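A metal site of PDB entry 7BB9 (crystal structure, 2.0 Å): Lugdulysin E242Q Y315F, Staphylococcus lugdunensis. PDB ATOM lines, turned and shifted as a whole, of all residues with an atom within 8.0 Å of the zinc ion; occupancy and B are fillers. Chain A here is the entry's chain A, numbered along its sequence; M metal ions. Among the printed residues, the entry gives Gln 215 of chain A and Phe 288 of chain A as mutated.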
ATOM      1  N   GLU A  45       5.105 -13.136   4.959  1.00  0.00           N
ATOM      2  CA  GLU A  45       4.254 -14.307   5.115  1.00  0.00           C
ATOM      3  C   GLU A  45       2.889 -13.917   5.674  1.00  0.00           C
ATOM      4  O   GLU A  45       2.636 -12.770   6.037  1.00  0.00           O
ATOM      5  CB  GLU A  45       4.856 -15.303   6.109  1.00  0.00           C
ATOM      6  CG  GLU A  45       5.926 -16.229   5.656  1.00  0.00           C
ATOM      7  CD  GLU A  45       6.190 -17.232   6.755  1.00  0.00           C
ATOM      8  OE1 GLU A  45       6.975 -16.935   7.669  1.00  0.00           O
ATOM      9  OE2 GLU A  45       5.548 -18.312   6.730  1.00  0.00           O
ATOM     10  N   ASP A  46       2.041 -14.935   5.821  1.00  0.00           N
ATOM     11  CA  ASP A  46       0.857 -14.876   6.660  1.00  0.00           C
ATOM     12  C   ASP A  46       0.544 -16.302   7.078  1.00  0.00           C
ATOM     13  O   ASP A  46       1.202 -17.246   6.656  1.00  0.00           O
ATOM     14  CB  ASP A  46      -0.320 -14.167   5.957  1.00  0.00           C
ATOM     15  CG  ASP A  46      -1.095 -15.070   5.030  1.00  0.00           C
ATOM     16  OD1 ASP A  46      -0.545 -15.437   3.970  1.00  0.00           O
ATOM     17  OD2 ASP A  46      -2.263 -15.396   5.335  1.00  0.00           O
ATOM     18  N   LYS A  47      -0.432 -16.443   7.977  1.00  0.00           N
ATOM     19  CA  LYS A  47      -0.815 -17.742   8.519  1.00  0.00           C
ATOM     20  C   LYS A  47      -2.299 -17.947   8.271  1.00  0.00           C
ATOM     21  O   LYS A  47      -3.120 -17.080   8.587  1.00  0.00           O
ATOM     22  CB  LYS A  47      -0.538 -17.855  10.025  1.00  0.00           C
ATOM     23  CG  LYS A  47       0.931 -17.793  10.425  1.00  0.00           C
ATOM     24  CD  LYS A  47       1.689 -19.084  10.166  1.00  0.00           C
ATOM     25  CE  LYS A  47       3.051 -19.061  10.860  1.00  0.00           C
ATOM     26  NZ  LYS A  47       4.165 -19.570  10.017  1.00  0.00           N
ATOM     27  N   LEU A  48      -2.621 -19.086   7.674  1.00  0.00           N
ATOM     28  CA  LEU A  48      -3.989 -19.573   7.549  1.00  0.00           C
ATOM     29  C   LEU A  48      -4.086 -20.795   8.437  1.00  0.00           C
ATOM     30  O   LEU A  48      -3.450 -21.818   8.162  1.00  0.00           O
ATOM     31  CB  LEU A  48      -4.321 -19.907   6.096  1.00  0.00           C
ATOM     32  CG  LEU A  48      -5.578 -20.746   5.873  1.00  0.00           C
ATOM     33  CD1 LEU A  48      -6.866 -19.950   6.193  1.00  0.00           C
ATOM     34  CD2 LEU A  48      -5.597 -21.277   4.456  1.00  0.00           C
ATOM     35  N   PHE A  49      -4.843 -20.687   9.508  1.00  0.00           N
ATOM     36  CA  PHE A  49      -4.966 -21.792  10.449  1.00  0.00           C
ATOM     37  C   PHE A  49      -6.120 -22.690  10.046  1.00  0.00           C
ATOM     38  O   PHE A  49      -7.011 -22.297   9.290  1.00  0.00           O
ATOM     39  CB  PHE A  49      -5.173 -21.256  11.873  1.00  0.00           C
ATOM     40  CG  PHE A  49      -4.005 -20.460  12.396  1.00  0.00           C
ATOM     41  CD1 PHE A  49      -2.956 -21.093  13.046  1.00  0.00           C
ATOM     42  CD2 PHE A  49      -3.945 -19.074  12.229  1.00  0.00           C
ATOM     43  CE1 PHE A  49      -1.874 -20.385  13.519  1.00  0.00           C
ATOM     44  CE2 PHE A  49      -2.876 -18.363  12.709  1.00  0.00           C
ATOM     45  CZ  PHE A  49      -1.829 -19.017  13.352  1.00  0.00           C
ATOM     46  N   GLY A 169      -0.472 -10.753   8.387  1.00  0.00           N
ATOM     47  CA  GLY A 169      -1.862 -10.908   8.784  1.00  0.00           C
ATOM     48  C   GLY A 169      -2.179 -12.374   8.965  1.00  0.00           C
ATOM     49  O   GLY A 169      -1.406 -13.250   8.563  1.00  0.00           O
ATOM     50  N   TYR A 170      -3.329 -12.652   9.596  1.00  0.00           N
ATOM     51  CA  TYR A 170      -3.748 -14.043   9.679  1.00  0.00           C
ATOM     52  C   TYR A 170      -5.264 -14.138   9.814  1.00  0.00           C
ATOM     53  O   TYR A 170      -5.953 -13.146  10.068  1.00  0.00           O
ATOM     54  CB  TYR A 170      -3.033 -14.791  10.805  1.00  0.00           C
ATOM     55  CG  TYR A 170      -3.335 -14.386  12.238  1.00  0.00           C
ATOM     56  CD1 TYR A 170      -2.606 -13.364  12.862  1.00  0.00           C
ATOM     57  CD2 TYR A 170      -4.293 -15.060  12.983  1.00  0.00           C
ATOM     58  CE1 TYR A 170      -2.851 -13.019  14.186  1.00  0.00           C
ATOM     59  CE2 TYR A 170      -4.538 -14.714  14.307  1.00  0.00           C
ATOM     60  CZ  TYR A 170      -3.819 -13.694  14.897  1.00  0.00           C
ATOM     61  OH  TYR A 170      -4.078 -13.349  16.195  1.00  0.00           O
ATOM     62  N   PHE A 171      -5.774 -15.358   9.601  1.00  0.00           N
ATOM     63  CA  PHE A 171      -7.173 -15.693   9.788  1.00  0.00           C
ATOM     64  C   PHE A 171      -7.263 -17.046  10.480  1.00  0.00           C
ATOM     65  O   PHE A 171      -6.509 -17.972  10.136  1.00  0.00           O
ATOM     66  CB  PHE A 171      -7.941 -15.748   8.457  1.00  0.00           C
ATOM     67  CG  PHE A 171      -9.383 -16.151   8.602  1.00  0.00           C
ATOM     68  CD1 PHE A 171     -10.328 -15.246   9.054  1.00  0.00           C
ATOM     69  CD2 PHE A 171      -9.794 -17.441   8.274  1.00  0.00           C
ATOM     70  CE1 PHE A 171     -11.655 -15.609   9.171  1.00  0.00           C
ATOM     71  CE2 PHE A 171     -11.117 -17.813   8.405  1.00  0.00           C
ATOM     72  CZ  PHE A 171     -12.055 -16.891   8.845  1.00  0.00           C
ATOM     73  N   THR A 211      -3.338  -6.657   1.564  1.00  0.00           N
ATOM     74  CA  THR A 211      -3.438  -7.719   2.557  1.00  0.00           C
ATOM     75  C   THR A 211      -4.851  -7.826   3.117  1.00  0.00           C
ATOM     76  O   THR A 211      -5.267  -8.915   3.533  1.00  0.00           O
ATOM     77  CB  THR A 211      -2.414  -7.496   3.674  1.00  0.00           C
ATOM     78  OG1 THR A 211      -1.109  -7.356   3.074  1.00  0.00           O
ATOM     79  CG2 THR A 211      -2.388  -8.671   4.673  1.00  0.00           C
ATOM     80  N   HIS A 214      -6.358 -10.112   0.777  1.00  0.00           N
ATOM     81  CA  HIS A 214      -5.817 -11.442   1.078  1.00  0.00           C
ATOM     82  C   HIS A 214      -6.559 -12.116   2.237  1.00  0.00           C
ATOM     83  O   HIS A 214      -7.114 -13.211   2.104  1.00  0.00           O
ATOM     84  CB  HIS A 214      -4.314 -11.319   1.379  1.00  0.00           C
ATOM     85  CG  HIS A 214      -3.656 -12.635   1.690  1.00  0.00           C
ATOM     86  ND1 HIS A 214      -2.614 -13.135   0.941  1.00  0.00           N
ATOM     87  CD2 HIS A 214      -3.889 -13.542   2.665  1.00  0.00           C
ATOM     88  CE1 HIS A 214      -2.227 -14.286   1.457  1.00  0.00           C
ATOM     89  NE2 HIS A 214      -2.989 -14.565   2.500  1.00  0.00           N
ATOM     90  N   GLN A 215      -6.586 -11.441   3.399  1.00  0.00           N
ATOM     91  CA  GLN A 215      -7.174 -12.068   4.574  1.00  0.00           C
ATOM     92  C   GLN A 215      -8.684 -12.232   4.427  1.00  0.00           C
ATOM     93  O   GLN A 215      -9.242 -13.226   4.909  1.00  0.00           O
ATOM     94  CB  GLN A 215      -6.833 -11.262   5.839  1.00  0.00           C
ATOM     95  CG  GLN A 215      -5.356 -11.339   6.226  1.00  0.00           C
ATOM     96  CD  GLN A 215      -4.868 -12.777   6.395  1.00  0.00           C
ATOM     97  OE1 GLN A 215      -5.615 -13.661   6.800  1.00  0.00           O
ATOM     98  NE2 GLN A 215      -3.603 -13.019   6.063  1.00  0.00           N
ATOM     99  N   GLN A 217     -10.324 -12.899   1.742  1.00  0.00           N
ATOM    100  CA  GLN A 217     -10.561 -14.088   0.924  1.00  0.00           C
ATOM    101  C   GLN A 217     -10.583 -15.352   1.789  1.00  0.00           C
ATOM    102  O   GLN A 217     -11.480 -16.186   1.650  1.00  0.00           O
ATOM    103  CB  GLN A 217      -9.503 -14.191  -0.176  1.00  0.00           C
ATOM    104  CG  GLN A 217      -9.829 -15.187  -1.282  1.00  0.00           C
ATOM    105  CD  GLN A 217      -9.659 -16.648  -0.852  1.00  0.00           C
ATOM    106  OE1 GLN A 217     -10.489 -17.501  -1.169  1.00  0.00           O
ATOM    107  NE2 GLN A 217      -8.577 -16.940  -0.155  1.00  0.00           N
ATOM    108  N   HIS A 218      -9.578 -15.519   2.661  1.00  0.00           N
ATOM    109  CA  HIS A 218      -9.579 -16.608   3.634  1.00  0.00           C
ATOM    110  C   HIS A 218     -10.909 -16.681   4.382  1.00  0.00           C
ATOM    111  O   HIS A 218     -11.453 -17.786   4.594  1.00  0.00           O
ATOM    112  CB  HIS A 218      -8.440 -16.417   4.643  1.00  0.00           C
ATOM    113  CG  HIS A 218      -7.071 -16.730   4.123  1.00  0.00           C
ATOM    114  ND1 HIS A 218      -6.823 -17.738   3.221  1.00  0.00           N
ATOM    115  CD2 HIS A 218      -5.861 -16.172   4.409  1.00  0.00           C
ATOM    116  CE1 HIS A 218      -5.524 -17.791   2.967  1.00  0.00           C
ATOM    117  NE2 HIS A 218      -4.920 -16.844   3.665  1.00  0.00           N
ATOM    118  N   PRO A 237      -4.660 -25.878   2.136  1.00  0.00           N
ATOM    119  CA  PRO A 237      -3.986 -24.577   2.327  1.00  0.00           C
ATOM    120  C   PRO A 237      -3.359 -24.013   1.060  1.00  0.00           C
ATOM    121  O   PRO A 237      -3.497 -22.808   0.797  1.00  0.00           O
ATOM    122  CB  PRO A 237      -2.915 -24.914   3.380  1.00  0.00           C
ATOM    123  CG  PRO A 237      -3.523 -26.097   4.151  1.00  0.00           C
ATOM    124  CD  PRO A 237      -4.239 -26.894   3.113  1.00  0.00           C
ATOM    125  N   ASN A 240      -6.087 -22.404  -1.036  1.00  0.00           N
ATOM    126  CA  ASN A 240      -6.635 -21.279  -0.288  1.00  0.00           C
ATOM    127  C   ASN A 240      -5.672 -20.100  -0.328  1.00  0.00           C
ATOM    128  O   ASN A 240      -6.057 -18.969  -0.669  1.00  0.00           O
ATOM    129  CB  ASN A 240      -6.933 -21.725   1.158  1.00  0.00           C
ATOM    130  CG  ASN A 240      -7.917 -20.809   1.861  1.00  0.00           C
ATOM    131  OD1 ASN A 240      -8.014 -19.631   1.553  1.00  0.00           O
ATOM    132  ND2 ASN A 240      -8.678 -21.358   2.831  1.00  0.00           N
ATOM    133  N   GLU A 241      -4.389 -20.339  -0.039  1.00  0.00           N
ATOM    134  CA  GLU A 241      -3.371 -19.294  -0.130  1.00  0.00           C
ATOM    135  C   GLU A 241      -3.230 -18.757  -1.567  1.00  0.00           C
ATOM    136  O   GLU A 241      -3.021 -17.559  -1.779  1.00  0.00           O
ATOM    137  CB  GLU A 241      -2.028 -19.820   0.383  1.00  0.00           C
ATOM    138  CG  GLU A 241      -1.994 -20.111   1.896  1.00  0.00           C
ATOM    139  CD  GLU A 241      -2.085 -18.848   2.740  1.00  0.00           C
ATOM    140  OE1 GLU A 241      -2.161 -18.937   3.999  1.00  0.00           O
ATOM    141  OE2 GLU A 241      -2.096 -17.758   2.155  1.00  0.00           O
ATOM    142  N   ALA A 242      -3.332 -19.639  -2.566  1.00  0.00           N
ATOM    143  CA  ALA A 242      -3.242 -19.165  -3.952  1.00  0.00           C
ATOM    144  C   ALA A 242      -4.373 -18.191  -4.280  1.00  0.00           C
ATOM    145  O   ALA A 242      -4.138 -17.148  -4.921  1.00  0.00           O
ATOM    146  CB  ALA A 242      -3.257 -20.338  -4.941  1.00  0.00           C
ATOM    147  N   LEU A 243      -5.597 -18.505  -3.835  1.00  0.00           N
ATOM    148  CA  LEU A 243      -6.736 -17.646  -4.111  1.00  0.00           C
ATOM    149  C   LEU A 243      -6.611 -16.300  -3.411  1.00  0.00           C
ATOM    150  O   LEU A 243      -7.036 -15.267  -3.947  1.00  0.00           O
ATOM    151  CB  LEU A 243      -8.045 -18.340  -3.709  1.00  0.00           C
ATOM    152  CG  LEU A 243      -8.546 -19.401  -4.683  1.00  0.00           C
ATOM    153  CD1 LEU A 243      -9.520 -20.377  -3.977  1.00  0.00           C
ATOM    154  CD2 LEU A 243      -9.170 -18.796  -5.945  1.00  0.00           C
ATOM    155  N   SER A 244      -6.015 -16.292  -2.207  1.00  0.00           N
ATOM    156  CA  SER A 244      -5.794 -15.022  -1.517  1.00  0.00           C
ATOM    157  C   SER A 244      -4.845 -14.121  -2.290  1.00  0.00           C
ATOM    158  O   SER A 244      -4.983 -12.899  -2.258  1.00  0.00           O
ATOM    159  CB  SER A 244      -5.256 -15.274  -0.107  1.00  0.00           C
ATOM    160  OG  SER A 244      -6.320 -15.550   0.782  1.00  0.00           O
ATOM    161  N   MET A 245      -3.868 -14.710  -2.966  1.00  0.00           N
ATOM    162  CA  MET A 245      -2.918 -13.909  -3.707  1.00  0.00           C
ATOM    163  C   MET A 245      -3.444 -13.541  -5.084  1.00  0.00           C
ATOM    164  O   MET A 245      -3.047 -12.517  -5.641  1.00  0.00           O
ATOM    165  CB  MET A 245      -1.578 -14.642  -3.759  1.00  0.00           C
ATOM    166  CG  MET A 245      -0.939 -14.726  -2.385  1.00  0.00           C
ATOM    167  SD  MET A 245       0.668 -15.535  -2.512  1.00  0.00           S
ATOM    168  CE  MET A 245       0.088 -17.218  -2.832  1.00  0.00           C
ATOM    169  N   GLU A 248      -5.110 -10.299  -4.233  1.00  0.00           N
ATOM    170  CA  GLU A 248      -4.195  -9.172  -4.128  1.00  0.00           C
ATOM    171  C   GLU A 248      -3.906  -8.590  -5.498  1.00  0.00           C
ATOM    172  O   GLU A 248      -3.988  -7.370  -5.694  1.00  0.00           O
ATOM    173  CB  GLU A 248      -2.892  -9.581  -3.427  1.00  0.00           C
ATOM    174  CG  GLU A 248      -3.099 -10.149  -2.035  1.00  0.00           C
ATOM    175  CD  GLU A 248      -1.805 -10.254  -1.250  1.00  0.00           C
ATOM    176  OE1 GLU A 248      -1.119  -9.221  -1.097  1.00  0.00           O
ATOM    177  OE2 GLU A 248      -1.482 -11.374  -0.780  1.00  0.00           O
ATOM    178  N   ARG A 259       6.648 -11.717  -5.067  1.00  0.00           N
ATOM    179  CA  ARG A 259       6.566 -13.176  -5.104  1.00  0.00           C
ATOM    180  C   ARG A 259       7.330 -13.757  -6.291  1.00  0.00           C
ATOM    181  O   ARG A 259       7.877 -14.866  -6.193  1.00  0.00           O
ATOM    182  CB  ARG A 259       5.105 -13.631  -5.157  1.00  0.00           C
ATOM    183  CG  ARG A 259       4.273 -13.179  -3.975  1.00  0.00           C
ATOM    184  CD  ARG A 259       4.695 -13.863  -2.671  1.00  0.00           C
ATOM    185  NE  ARG A 259       3.811 -13.452  -1.582  1.00  0.00           N
ATOM    186  CZ  ARG A 259       4.130 -13.510  -0.297  1.00  0.00           C
ATOM    187  NH1 ARG A 259       5.311 -13.980   0.093  1.00  0.00           N
ATOM    188  NH2 ARG A 259       3.261 -13.116   0.610  1.00  0.00           N
ATOM    189  N   TRP A 278       2.308 -27.840   1.986  1.00  0.00           N
ATOM    190  CA  TRP A 278       2.677 -26.590   2.638  1.00  0.00           C
ATOM    191  C   TRP A 278       3.720 -26.866   3.713  1.00  0.00           C
ATOM    192  O   TRP A 278       3.421 -27.513   4.722  1.00  0.00           O
ATOM    193  CB  TRP A 278       1.449 -25.906   3.253  1.00  0.00           C
ATOM    194  CG  TRP A 278       1.560 -24.393   3.363  1.00  0.00           C
ATOM    195  CD1 TRP A 278       1.840 -23.673   4.500  1.00  0.00           C
ATOM    196  CD2 TRP A 278       1.400 -23.442   2.306  1.00  0.00           C
ATOM    197  NE1 TRP A 278       1.849 -22.321   4.208  1.00  0.00           N
ATOM    198  CE2 TRP A 278       1.593 -22.151   2.866  1.00  0.00           C
ATOM    199  CE3 TRP A 278       1.109 -23.535   0.943  1.00  0.00           C
ATOM    200  CZ2 TRP A 278       1.514 -20.993   2.110  1.00  0.00           C
ATOM    201  CZ3 TRP A 278       1.027 -22.387   0.188  1.00  0.00           C
ATOM    202  CH2 TRP A 278       1.235 -21.127   0.781  1.00  0.00           C
ATOM    203  N   PHE A 288       4.340 -19.698  -0.939  1.00  0.00           N
ATOM    204  CA  PHE A 288       3.598 -18.537  -1.414  1.00  0.00           C
ATOM    205  C   PHE A 288       3.925 -18.224  -2.867  1.00  0.00           C
ATOM    206  O   PHE A 288       3.024 -17.937  -3.658  1.00  0.00           O
ATOM    207  CB  PHE A 288       3.882 -17.327  -0.502  1.00  0.00           C
ATOM    208  CG  PHE A 288       3.182 -17.408   0.827  1.00  0.00           C
ATOM    209  CD1 PHE A 288       1.813 -17.268   0.894  1.00  0.00           C
ATOM    210  CD2 PHE A 288       3.885 -17.669   2.000  1.00  0.00           C
ATOM    211  CE1 PHE A 288       1.135 -17.368   2.116  1.00  0.00           C
ATOM    212  CE2 PHE A 288       3.228 -17.775   3.219  1.00  0.00           C
ATOM    213  CZ  PHE A 288       1.858 -17.635   3.286  1.00  0.00           C
HETATM  214 ZN    ZN M   1      -2.913 -16.356   3.489  1.00  0.00          ZN
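The backbone carbonyl oxygen of His 214 is in hydrogen-bond range of the side-chain hydroxyl of Ser 244 (2.8 Å). A ring nitrogen (ND1) of His 214 lies within hydrogen-bond range of the side-chain carboxylate (OE2) of Glu 248 (2.7 Å). ND1 of His 218 lies close to OG of Ser 244. ND1 of His 218 lies within hydrogen-bond range of OD1 of Asn 240, at 2.8 Å. The side-chain carboxylate (OD2) of Asp 46 sits close to the side-chain amide nitrogen (NE2) of Gln 215 (2.8 Å).
The zinc ion is bound by NE2 of His 214, NE2 of His 218, OE2 of Glu 241, OD2 of Asp 46 and OD1 of Asp 46. The zinc ion has five donor atoms within binding distance. Slightly farther from the zinc ion lies OE1 of Glu 241 (2.7 Å).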
